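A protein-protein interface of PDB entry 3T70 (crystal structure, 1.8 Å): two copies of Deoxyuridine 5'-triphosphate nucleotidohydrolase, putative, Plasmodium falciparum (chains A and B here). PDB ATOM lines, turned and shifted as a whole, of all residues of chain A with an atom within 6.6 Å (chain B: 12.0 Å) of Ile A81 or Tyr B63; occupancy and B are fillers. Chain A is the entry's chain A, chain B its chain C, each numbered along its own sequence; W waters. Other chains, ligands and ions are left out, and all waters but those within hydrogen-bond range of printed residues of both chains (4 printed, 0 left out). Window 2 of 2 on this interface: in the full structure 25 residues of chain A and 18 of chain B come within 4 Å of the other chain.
Of chain B, only Tyr B63 (3.6 Å) and Lys B65 (3.5 Å) come within 4 Å of His A2. No residue of chain B comes within 4 Å of Asn A80. Ile A81 touches one residue of chain B. No residue of chain B comes within 4 Å of Val A82. Printed residues of chain B within 4 Å of Glu A150: Lys B65. Of the printed residues of chain A, Tyr B62 touches Tyr A58 (3.4 Å), Glu A145 (3.0 Å) and Pro A146 (3.7 Å). Printed residues of chain A within 4 Å of Tyr B63: Met A1 (2.7 Å), His A2 (3.6 Å), Leu A56 (3.7 Å), Tyr A58 (3.4 Å) and Ile A81 (3.5 Å). Printed residues of chain A within 4 Å of Lys B65: His A2 (3.5 Å), Ser A148 (2.8 Å) and Glu A150 (3.999 Å). The nearest residue of chain B that does not touch Ile A81 is Lys B65 (7.4 Å). The nearest printed residue of chain A that does not touch Tyr B63 is Gln A57 (4.2 Å).
Printed residues of chain B that touch a printed residue of chain A: Asn B61, Tyr B62, Tyr B63, Tyr B64 and Lys B65. Among the printed residues, 15 pairs touch across the chains.
Water W2 lies within hydrogen-bond range of the side-chain carboxylate of Glu A150 (2.6 Å) and the side-chain amino group of Lys B65 (2.8 Å). Water W4 bridges OE2 of Glu A145 (2.7 Å) and OG of Ser B60 (3.2 Å). Water W1 lies within hydrogen-bond range of the backbone NH (N) of Tyr B64 (2.9 Å), the side-chain hydroxyl (OH) of Tyr A58 (3.2 Å) and the backbone carbonyl oxygen (O) of Tyr B62 (3.2 Å). Water W3 lies within hydrogen-bond range of OE1 of Glu A145 (2.9 Å), N of Tyr B63 (3.2 Å) and N of Tyr A58 (3.3 Å).
A ring nitrogen (ND1) of His A2 sits at hydrogen-bond distance from the side-chain hydroxyl of Ser A148, at 2.7 Å. A ring nitrogen (NE2) of His A2 lies within hydrogen-bond range of the side-chain carboxylate of Glu A150. The backbone NH (N) of Met A1 sits at hydrogen-bond distance from the backbone carbonyl oxygen (O) of Pro A146 (3.0 Å). The backbone carbonyl oxygen of His A2 sits at hydrogen-bond distance from the backbone NH of Leu A56. The backbone NH of Met A1 lies within hydrogen-bond range of the side-chain carboxylate of Glu A145, at 2.7 Å. The backbone NH (N) of Ser A148 lies within hydrogen-bond range of the backbone carbonyl oxygen (O) of Met A1 (3.1 Å).
His A2 touches Tyr B63. Lys B65 touches His A2. CD1 of Tyr A58 touches O of Asn B61 (3.98 Å). Tyr A58 touches Tyr B62 (CE1 to C, 3.4 Å). Glu A145 touches Tyr B62. Pro A146 touches Tyr B62 (CG to OH, 3.7 Å). O of Pro A146 touches CD1 of Tyr B64, at 3.7 Å. Tyr B64 touches Leu A147 (CE1 to O, 3.5 Å). Ser A148 touches Tyr B64. Glu A150 touches Lys B65.
Position printed for both chains: 59. Of the 15 pairs that touch across the chains among the printed residues, none has its exchanged pair printed and touching as well.
The backbone NH of Met A1 sits at hydrogen-bond distance from the backbone carbonyl oxygen of Tyr B63, at 2.7 Å. OG of Ser A148 lies within hydrogen-bond range of N of Lys B65, 2.8 Å away.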
ATOM      1  N   MET A   1      10.491  26.940  -7.936  1.00  0.00           N
ATOM      2  CA  MET A   1      10.496  27.215  -6.470  1.00  0.00           C
ATOM      3  C   MET A   1      11.550  26.338  -5.815  1.00  0.00           C
ATOM      4  O   MET A   1      11.731  25.184  -6.203  1.00  0.00           O
ATOM      5  CB  MET A   1       9.115  26.939  -5.859  1.00  0.00           C
ATOM      6  CG  MET A   1       8.964  27.369  -4.397  1.00  0.00           C
ATOM      7  SD  MET A   1       7.326  27.041  -3.707  1.00  0.00           S
ATOM      8  CE  MET A   1       7.440  25.302  -3.290  1.00  0.00           C
ATOM      9  N   HIS A   2      12.240  26.883  -4.821  1.00  0.00           N
ATOM     10  CA  HIS A   2      13.296  26.145  -4.148  1.00  0.00           C
ATOM     11  C   HIS A   2      12.995  25.981  -2.662  1.00  0.00           C
ATOM     12  O   HIS A   2      12.712  26.957  -1.971  1.00  0.00           O
ATOM     13  CB  HIS A   2      14.643  26.852  -4.336  1.00  0.00           C
ATOM     14  CG  HIS A   2      15.786  26.153  -3.671  1.00  0.00           C
ATOM     15  ND1 HIS A   2      16.214  24.899  -4.051  1.00  0.00           N
ATOM     16  CD2 HIS A   2      16.600  26.538  -2.659  1.00  0.00           C
ATOM     17  CE1 HIS A   2      17.234  24.536  -3.292  1.00  0.00           C
ATOM     18  NE2 HIS A   2      17.489  25.514  -2.440  1.00  0.00           N
ATOM     19  N   LYS A   4      14.146  24.879   1.160  1.00  0.00           N
ATOM     20  CA  LYS A   4      15.177  24.558   2.144  1.00  0.00           C
ATOM     21  C   LYS A   4      14.531  23.710   3.234  1.00  0.00           C
ATOM     22  O   LYS A   4      13.571  24.140   3.882  1.00  0.00           O
ATOM     23  CB  LYS A   4      15.823  25.828   2.694  1.00  0.00           C
ATOM     24  CG  LYS A   4      16.634  26.590   1.623  1.00  0.00           C
ATOM     25  CD  LYS A   4      17.420  27.744   2.241  1.00  0.00           C
ATOM     26  CE  LYS A   4      18.299  28.414   1.190  1.00  0.00           C
ATOM     27  NZ  LYS A   4      19.035  29.603   1.728  1.00  0.00           N
ATOM     28  N   LEU A  56      11.328  29.225  -1.376  1.00  0.00           N
ATOM     29  CA  LEU A  56      11.914  30.432  -1.939  1.00  0.00           C
ATOM     30  C   LEU A  56      11.489  30.618  -3.389  1.00  0.00           C
ATOM     31  O   LEU A  56      11.521  29.673  -4.171  1.00  0.00           O
ATOM     32  CB  LEU A  56      13.436  30.371  -1.816  1.00  0.00           C
ATOM     33  CG  LEU A  56      13.960  30.329  -0.376  1.00  0.00           C
ATOM     34  CD1 LEU A  56      15.430  29.988  -0.352  1.00  0.00           C
ATOM     35  CD2 LEU A  56      13.723  31.671   0.289  1.00  0.00           C
ATOM     36  N   GLN A  57      11.071  31.840  -3.725  1.00  0.00           N
ATOM     37  CA  GLN A  57      10.700  32.218  -5.094  1.00  0.00           C
ATOM     38  C   GLN A  57      11.246  33.603  -5.420  1.00  0.00           C
ATOM     39  O   GLN A  57      11.692  34.326  -4.525  1.00  0.00           O
ATOM     40  CB  GLN A  57       9.180  32.232  -5.272  1.00  0.00           C
ATOM     41  CG  GLN A  57       8.562  30.859  -5.523  1.00  0.00           C
ATOM     42  CD  GLN A  57       7.027  30.840  -5.440  1.00  0.00           C
ATOM     43  OE1 GLN A  57       6.422  29.770  -5.342  1.00  0.00           O
ATOM     44  NE2 GLN A  57       6.400  32.019  -5.477  1.00  0.00           N
ATOM     45  N   TYR A  58      11.212  33.969  -6.698  1.00  0.00           N
ATOM     46  CA  TYR A  58      11.531  35.338  -7.097  1.00  0.00           C
ATOM     47  C   TYR A  58      10.463  36.287  -6.591  1.00  0.00           C
ATOM     48  O   TYR A  58       9.265  35.984  -6.651  1.00  0.00           O
ATOM     49  CB  TYR A  58      11.657  35.461  -8.614  1.00  0.00           C
ATOM     50  CG  TYR A  58      12.893  34.802  -9.162  1.00  0.00           C
ATOM     51  CD1 TYR A  58      12.830  33.998 -10.296  1.00  0.00           C
ATOM     52  CD2 TYR A  58      14.130  34.967  -8.534  1.00  0.00           C
ATOM     53  CE1 TYR A  58      13.966  33.390 -10.801  1.00  0.00           C
ATOM     54  CE2 TYR A  58      15.272  34.363  -9.029  1.00  0.00           C
ATOM     55  CZ  TYR A  58      15.182  33.576 -10.161  1.00  0.00           C
ATOM     56  OH  TYR A  58      16.309  32.974 -10.650  1.00  0.00           O
ATOM     57  N   LYS A  59      10.908  37.436  -6.090  1.00  0.00           N
ATOM     58  CA  LYS A  59      10.009  38.496  -5.672  1.00  0.00           C
ATOM     59  C   LYS A  59       9.144  38.921  -6.853  1.00  0.00           C
ATOM     60  O   LYS A  59       9.624  38.989  -7.987  1.00  0.00           O
ATOM     61  CB  LYS A  59      10.814  39.684  -5.134  1.00  0.00           C
ATOM     62  CG  LYS A  59       9.974  40.824  -4.566  1.00  0.00           C
ATOM     63  CD  LYS A  59      10.852  41.952  -4.049  1.00  0.00           C
ATOM     64  CE  LYS A  59      10.016  43.083  -3.474  1.00  0.00           C
ATOM     65  NZ  LYS A  59      10.864  44.195  -2.961  1.00  0.00           N
ATOM     66  N   ASN A  80      16.117  39.844  -4.158  1.00  0.00           N
ATOM     67  CA  ASN A  80      15.560  39.229  -5.363  1.00  0.00           C
ATOM     68  C   ASN A  80      14.718  37.985  -5.063  1.00  0.00           C
ATOM     69  O   ASN A  80      13.733  37.697  -5.752  1.00  0.00           O
ATOM     70  CB  ASN A  80      16.681  38.857  -6.340  1.00  0.00           C
ATOM     71  CG  ASN A  80      16.153  38.456  -7.709  1.00  0.00           C
ATOM     72  OD1 ASN A  80      15.095  38.926  -8.138  1.00  0.00           O
ATOM     73  ND2 ASN A  80      16.886  37.580  -8.401  1.00  0.00           N
ATOM     74  N   ILE A  81      15.129  37.252  -4.036  1.00  0.00           N
ATOM     75  CA  ILE A  81      14.493  35.995  -3.656  1.00  0.00           C
ATOM     76  C   ILE A  81      13.770  36.197  -2.328  1.00  0.00           C
ATOM     77  O   ILE A  81      14.314  36.807  -1.402  1.00  0.00           O
ATOM     78  CB  ILE A  81      15.543  34.865  -3.560  1.00  0.00           C
ATOM     79  CG1 ILE A  81      16.048  34.500  -4.959  1.00  0.00           C
ATOM     80  CG2 ILE A  81      14.974  33.625  -2.884  1.00  0.00           C
ATOM     81  CD1 ILE A  81      17.491  34.027  -4.983  1.00  0.00           C
ATOM     82  N   VAL A  82      12.537  35.702  -2.248  1.00  0.00           N
ATOM     83  CA  VAL A  82      11.724  35.857  -1.043  1.00  0.00           C
ATOM     84  C   VAL A  82      11.141  34.523  -0.563  1.00  0.00           C
ATOM     85  O   VAL A  82      10.869  33.633  -1.374  1.00  0.00           O
ATOM     86  CB  VAL A  82      10.571  36.896  -1.236  1.00  0.00           C
ATOM     87  CG1 VAL A  82      11.131  38.323  -1.373  1.00  0.00           C
ATOM     88  CG2 VAL A  82       9.676  36.540  -2.429  1.00  0.00           C
ATOM     89  N   ASN A  83      10.979  34.406   0.758  1.00  0.00           N
ATOM     90  CA  ASN A  83      10.192  33.343   1.394  1.00  0.00           C
ATOM     91  C   ASN A  83       8.745  33.444   0.924  1.00  0.00           C
ATOM     92  O   ASN A  83       8.153  34.527   0.961  1.00  0.00           O
ATOM     93  CB  ASN A  83      10.191  33.516   2.920  1.00  0.00           C
ATOM     94  CG  ASN A  83      11.325  32.788   3.608  1.00  0.00           C
ATOM     95  OD1 ASN A  83      11.205  32.411   4.779  1.00  0.00           O
ATOM     96  ND2 ASN A  83      12.429  32.582   2.902  1.00  0.00           N
ATOM     97  N   GLU A 145       5.378  25.653 -10.823  1.00  0.00           N
ATOM     98  CA  GLU A 145       6.696  25.469 -11.443  1.00  0.00           C
ATOM     99  C   GLU A 145       7.442  24.277 -10.831  1.00  0.00           C
ATOM    100  O   GLU A 145       7.084  23.823  -9.739  1.00  0.00           O
ATOM    101  CB  GLU A 145       7.530  26.758 -11.312  1.00  0.00           C
ATOM    102  CG  GLU A 145       8.046  27.051  -9.895  1.00  0.00           C
ATOM    103  CD  GLU A 145       8.224  28.541  -9.602  1.00  0.00           C
ATOM    104  OE1 GLU A 145       8.758  28.872  -8.533  1.00  0.00           O
ATOM    105  OE2 GLU A 145       7.815  29.385 -10.428  1.00  0.00           O
ATOM    106  N   PRO A 146       8.472  23.757 -11.536  1.00  0.00           N
ATOM    107  CA  PRO A 146       9.353  22.719 -10.979  1.00  0.00           C
ATOM    108  C   PRO A 146       9.947  23.084  -9.613  1.00  0.00           C
ATOM    109  O   PRO A 146      10.216  24.262  -9.328  1.00  0.00           O
ATOM    110  CB  PRO A 146      10.474  22.614 -12.022  1.00  0.00           C
ATOM    111  CG  PRO A 146       9.828  23.007 -13.288  1.00  0.00           C
ATOM    112  CD  PRO A 146       8.853  24.082 -12.930  1.00  0.00           C
ATOM    113  N   LEU A 147      10.131  22.070  -8.778  1.00  0.00           N
ATOM    114  CA  LEU A 147      10.653  22.275  -7.435  1.00  0.00           C
ATOM    115  C   LEU A 147      12.027  21.661  -7.294  1.00  0.00           C
ATOM    116  O   LEU A 147      12.255  20.520  -7.712  1.00  0.00           O
ATOM    117  CB  LEU A 147       9.730  21.646  -6.387  1.00  0.00           C
ATOM    118  CG  LEU A 147       8.260  22.036  -6.295  1.00  0.00           C
ATOM    119  CD1 LEU A 147       7.795  21.665  -4.908  1.00  0.00           C
ATOM    120  CD2 LEU A 147       8.000  23.513  -6.565  1.00  0.00           C
ATOM    121  N   SER A 148      12.939  22.422  -6.707  1.00  0.00           N
ATOM    122  CA  SER A 148      14.220  21.881  -6.261  1.00  0.00           C
ATOM    123  C   SER A 148      14.242  21.982  -4.744  1.00  0.00           C
ATOM    124  O   SER A 148      13.459  22.730  -4.159  1.00  0.00           O
ATOM    125  CB  SER A 148      15.391  22.663  -6.867  1.00  0.00           C
ATOM    126  OG  SER A 148      15.346  24.035  -6.511  1.00  0.00           O
ATOM    127  N   GLU A 150      17.037  21.579  -1.039  1.00  0.00           N
ATOM    128  CA  GLU A 150      18.302  21.270  -0.389  1.00  0.00           C
ATOM    129  C   GLU A 150      18.047  21.027   1.088  1.00  0.00           C
ATOM    130  O   GLU A 150      17.049  21.517   1.652  1.00  0.00           O
ATOM    131  CB  GLU A 150      19.317  22.399  -0.581  1.00  0.00           C
ATOM    132  CG  GLU A 150      18.955  23.699   0.117  1.00  0.00           C
ATOM    133  CD  GLU A 150      19.982  24.790  -0.102  1.00  0.00           C
ATOM    134  OE1 GLU A 150      21.089  24.695   0.479  1.00  0.00           O
ATOM    135  OE2 GLU A 150      19.679  25.745  -0.844  1.00  0.00           O
ATOM    136  N   LYS B  59       6.188  31.498 -21.200  1.00  0.00           N
ATOM    137  CA  LYS B  59       7.306  31.157 -20.334  1.00  0.00           C
ATOM    138  C   LYS B  59       7.474  32.227 -19.267  1.00  0.00           C
ATOM    139  O   LYS B  59       7.286  33.419 -19.529  1.00  0.00           O
ATOM    140  CB  LYS B  59       8.596  31.019 -21.146  1.00  0.00           C
ATOM    141  CG  LYS B  59       9.720  30.273 -20.425  1.00  0.00           C
ATOM    142  CD  LYS B  59      11.070  30.475 -21.110  1.00  0.00           C
ATOM    143  CE  LYS B  59      11.272  29.519 -22.278  1.00  0.00           C
ATOM    144  NZ  LYS B  59      12.586  29.728 -22.947  1.00  0.00           N
ATOM    145  N   SER B  60       7.808  31.783 -18.059  1.00  0.00           N
ATOM    146  CA  SER B  60       8.078  32.684 -16.951  1.00  0.00           C
ATOM    147  C   SER B  60       9.345  32.231 -16.247  1.00  0.00           C
ATOM    148  O   SER B  60       9.622  31.029 -16.169  1.00  0.00           O
ATOM    149  CB  SER B  60       6.905  32.707 -15.970  1.00  0.00           C
ATOM    150  OG  SER B  60       6.696  31.431 -15.388  1.00  0.00           O
ATOM    151  N   ASN B  61      10.126  33.195 -15.762  1.00  0.00           N
ATOM    152  CA  ASN B  61      11.320  32.893 -14.978  1.00  0.00           C
ATOM    153  C   ASN B  61      10.945  32.362 -13.601  1.00  0.00           C
ATOM    154  O   ASN B  61      10.059  32.904 -12.937  1.00  0.00           O
ATOM    155  CB  ASN B  61      12.249  34.113 -14.864  1.00  0.00           C
ATOM    156  CG  ASN B  61      11.496  35.420 -14.641  1.00  0.00           C
ATOM    157  OD1 ASN B  61      11.590  36.343 -15.453  1.00  0.00           O
ATOM    158  ND2 ASN B  61      10.747  35.505 -13.544  1.00  0.00           N
ATOM    159  N   TYR B  62      11.615  31.296 -13.185  1.00  0.00           N
ATOM    160  CA  TYR B  62      11.325  30.681 -11.899  1.00  0.00           C
ATOM    161  C   TYR B  62      12.593  30.271 -11.180  1.00  0.00           C
ATOM    162  O   TYR B  62      13.548  29.807 -11.810  1.00  0.00           O
ATOM    163  CB  TYR B  62      10.374  29.485 -12.063  1.00  0.00           C
ATOM    164  CG  TYR B  62      10.914  28.313 -12.858  1.00  0.00           C
ATOM    165  CD1 TYR B  62      10.702  28.224 -14.234  1.00  0.00           C
ATOM    166  CD2 TYR B  62      11.611  27.280 -12.230  1.00  0.00           C
ATOM    167  CE1 TYR B  62      11.185  27.142 -14.965  1.00  0.00           C
ATOM    168  CE2 TYR B  62      12.103  26.200 -12.954  1.00  0.00           C
ATOM    169  CZ  TYR B  62      11.881  26.137 -14.318  1.00  0.00           C
ATOM    170  OH  TYR B  62      12.363  25.069 -15.034  1.00  0.00           O
ATOM    171  N   TYR B  63      12.587  30.438  -9.860  1.00  0.00           N
ATOM    172  CA  TYR B  63      13.744  30.114  -9.031  1.00  0.00           C
ATOM    173  C   TYR B  63      13.879  28.606  -8.813  1.00  0.00           C
ATOM    174  O   TYR B  63      12.944  27.947  -8.358  1.00  0.00           O
ATOM    175  CB  TYR B  63      13.680  30.866  -7.698  1.00  0.00           C
ATOM    176  CG  TYR B  63      14.939  30.727  -6.870  1.00  0.00           C
ATOM    177  CD1 TYR B  63      16.185  31.099  -7.387  1.00  0.00           C
ATOM    178  CD2 TYR B  63      14.886  30.229  -5.570  1.00  0.00           C
ATOM    179  CE1 TYR B  63      17.345  30.970  -6.630  1.00  0.00           C
ATOM    180  CE2 TYR B  63      16.039  30.101  -4.803  1.00  0.00           C
ATOM    181  CZ  TYR B  63      17.266  30.470  -5.341  1.00  0.00           C
ATOM    182  OH  TYR B  63      18.407  30.338  -4.584  1.00  0.00           O
ATOM    183  N   TYR B  64      15.055  28.074  -9.140  1.00  0.00           N
ATOM    184  CA  TYR B  64      15.302  26.633  -9.126  1.00  0.00           C
ATOM    185  C   TYR B  64      16.803  26.383  -9.018  1.00  0.00           C
ATOM    186  O   TYR B  64      17.591  26.979  -9.764  1.00  0.00           O
ATOM    187  CB  TYR B  64      14.746  26.001 -10.412  1.00  0.00           C
ATOM    188  CG  TYR B  64      14.858  24.492 -10.505  1.00  0.00           C
ATOM    189  CD1 TYR B  64      13.798  23.668 -10.121  1.00  0.00           C
ATOM    190  CD2 TYR B  64      16.017  23.887 -11.006  1.00  0.00           C
ATOM    191  CE1 TYR B  64      13.889  22.280 -10.221  1.00  0.00           C
ATOM    192  CE2 TYR B  64      16.119  22.502 -11.106  1.00  0.00           C
ATOM    193  CZ  TYR B  64      15.052  21.706 -10.711  1.00  0.00           C
ATOM    194  OH  TYR B  64      15.152  20.334 -10.806  1.00  0.00           O
ATOM    195  N   LYS B  65      17.197  25.507  -8.094  1.00  0.00           N
ATOM    196  CA  LYS B  65      18.616  25.203  -7.877  1.00  0.00           C
ATOM    197  C   LYS B  65      18.996  23.822  -8.402  1.00  0.00           C
ATOM    198  O   LYS B  65      18.574  22.797  -7.867  1.00  0.00           O
ATOM    199  CB  LYS B  65      18.993  25.339  -6.399  1.00  0.00           C
ATOM    200  CG  LYS B  65      18.813  26.743  -5.834  1.00  0.00           C
ATOM    201  CD  LYS B  65      19.736  26.986  -4.645  1.00  0.00           C
ATOM    202  CE  LYS B  65      21.123  27.426  -5.097  1.00  0.00           C
ATOM    203  NZ  LYS B  65      21.989  27.830  -3.946  1.00  0.00           N
HETATM  204  O   HOH W   1      16.652  29.763 -10.880  1.00  0.00           O
HETATM  205  O   HOH W   2      20.577  28.073  -1.590  1.00  0.00           O
HETATM  206  O   HOH W   3       9.870  31.577  -8.616  1.00  0.00           O
HETATM  207  O   HOH W   4       7.005  31.268 -12.173  1.00  0.00           O
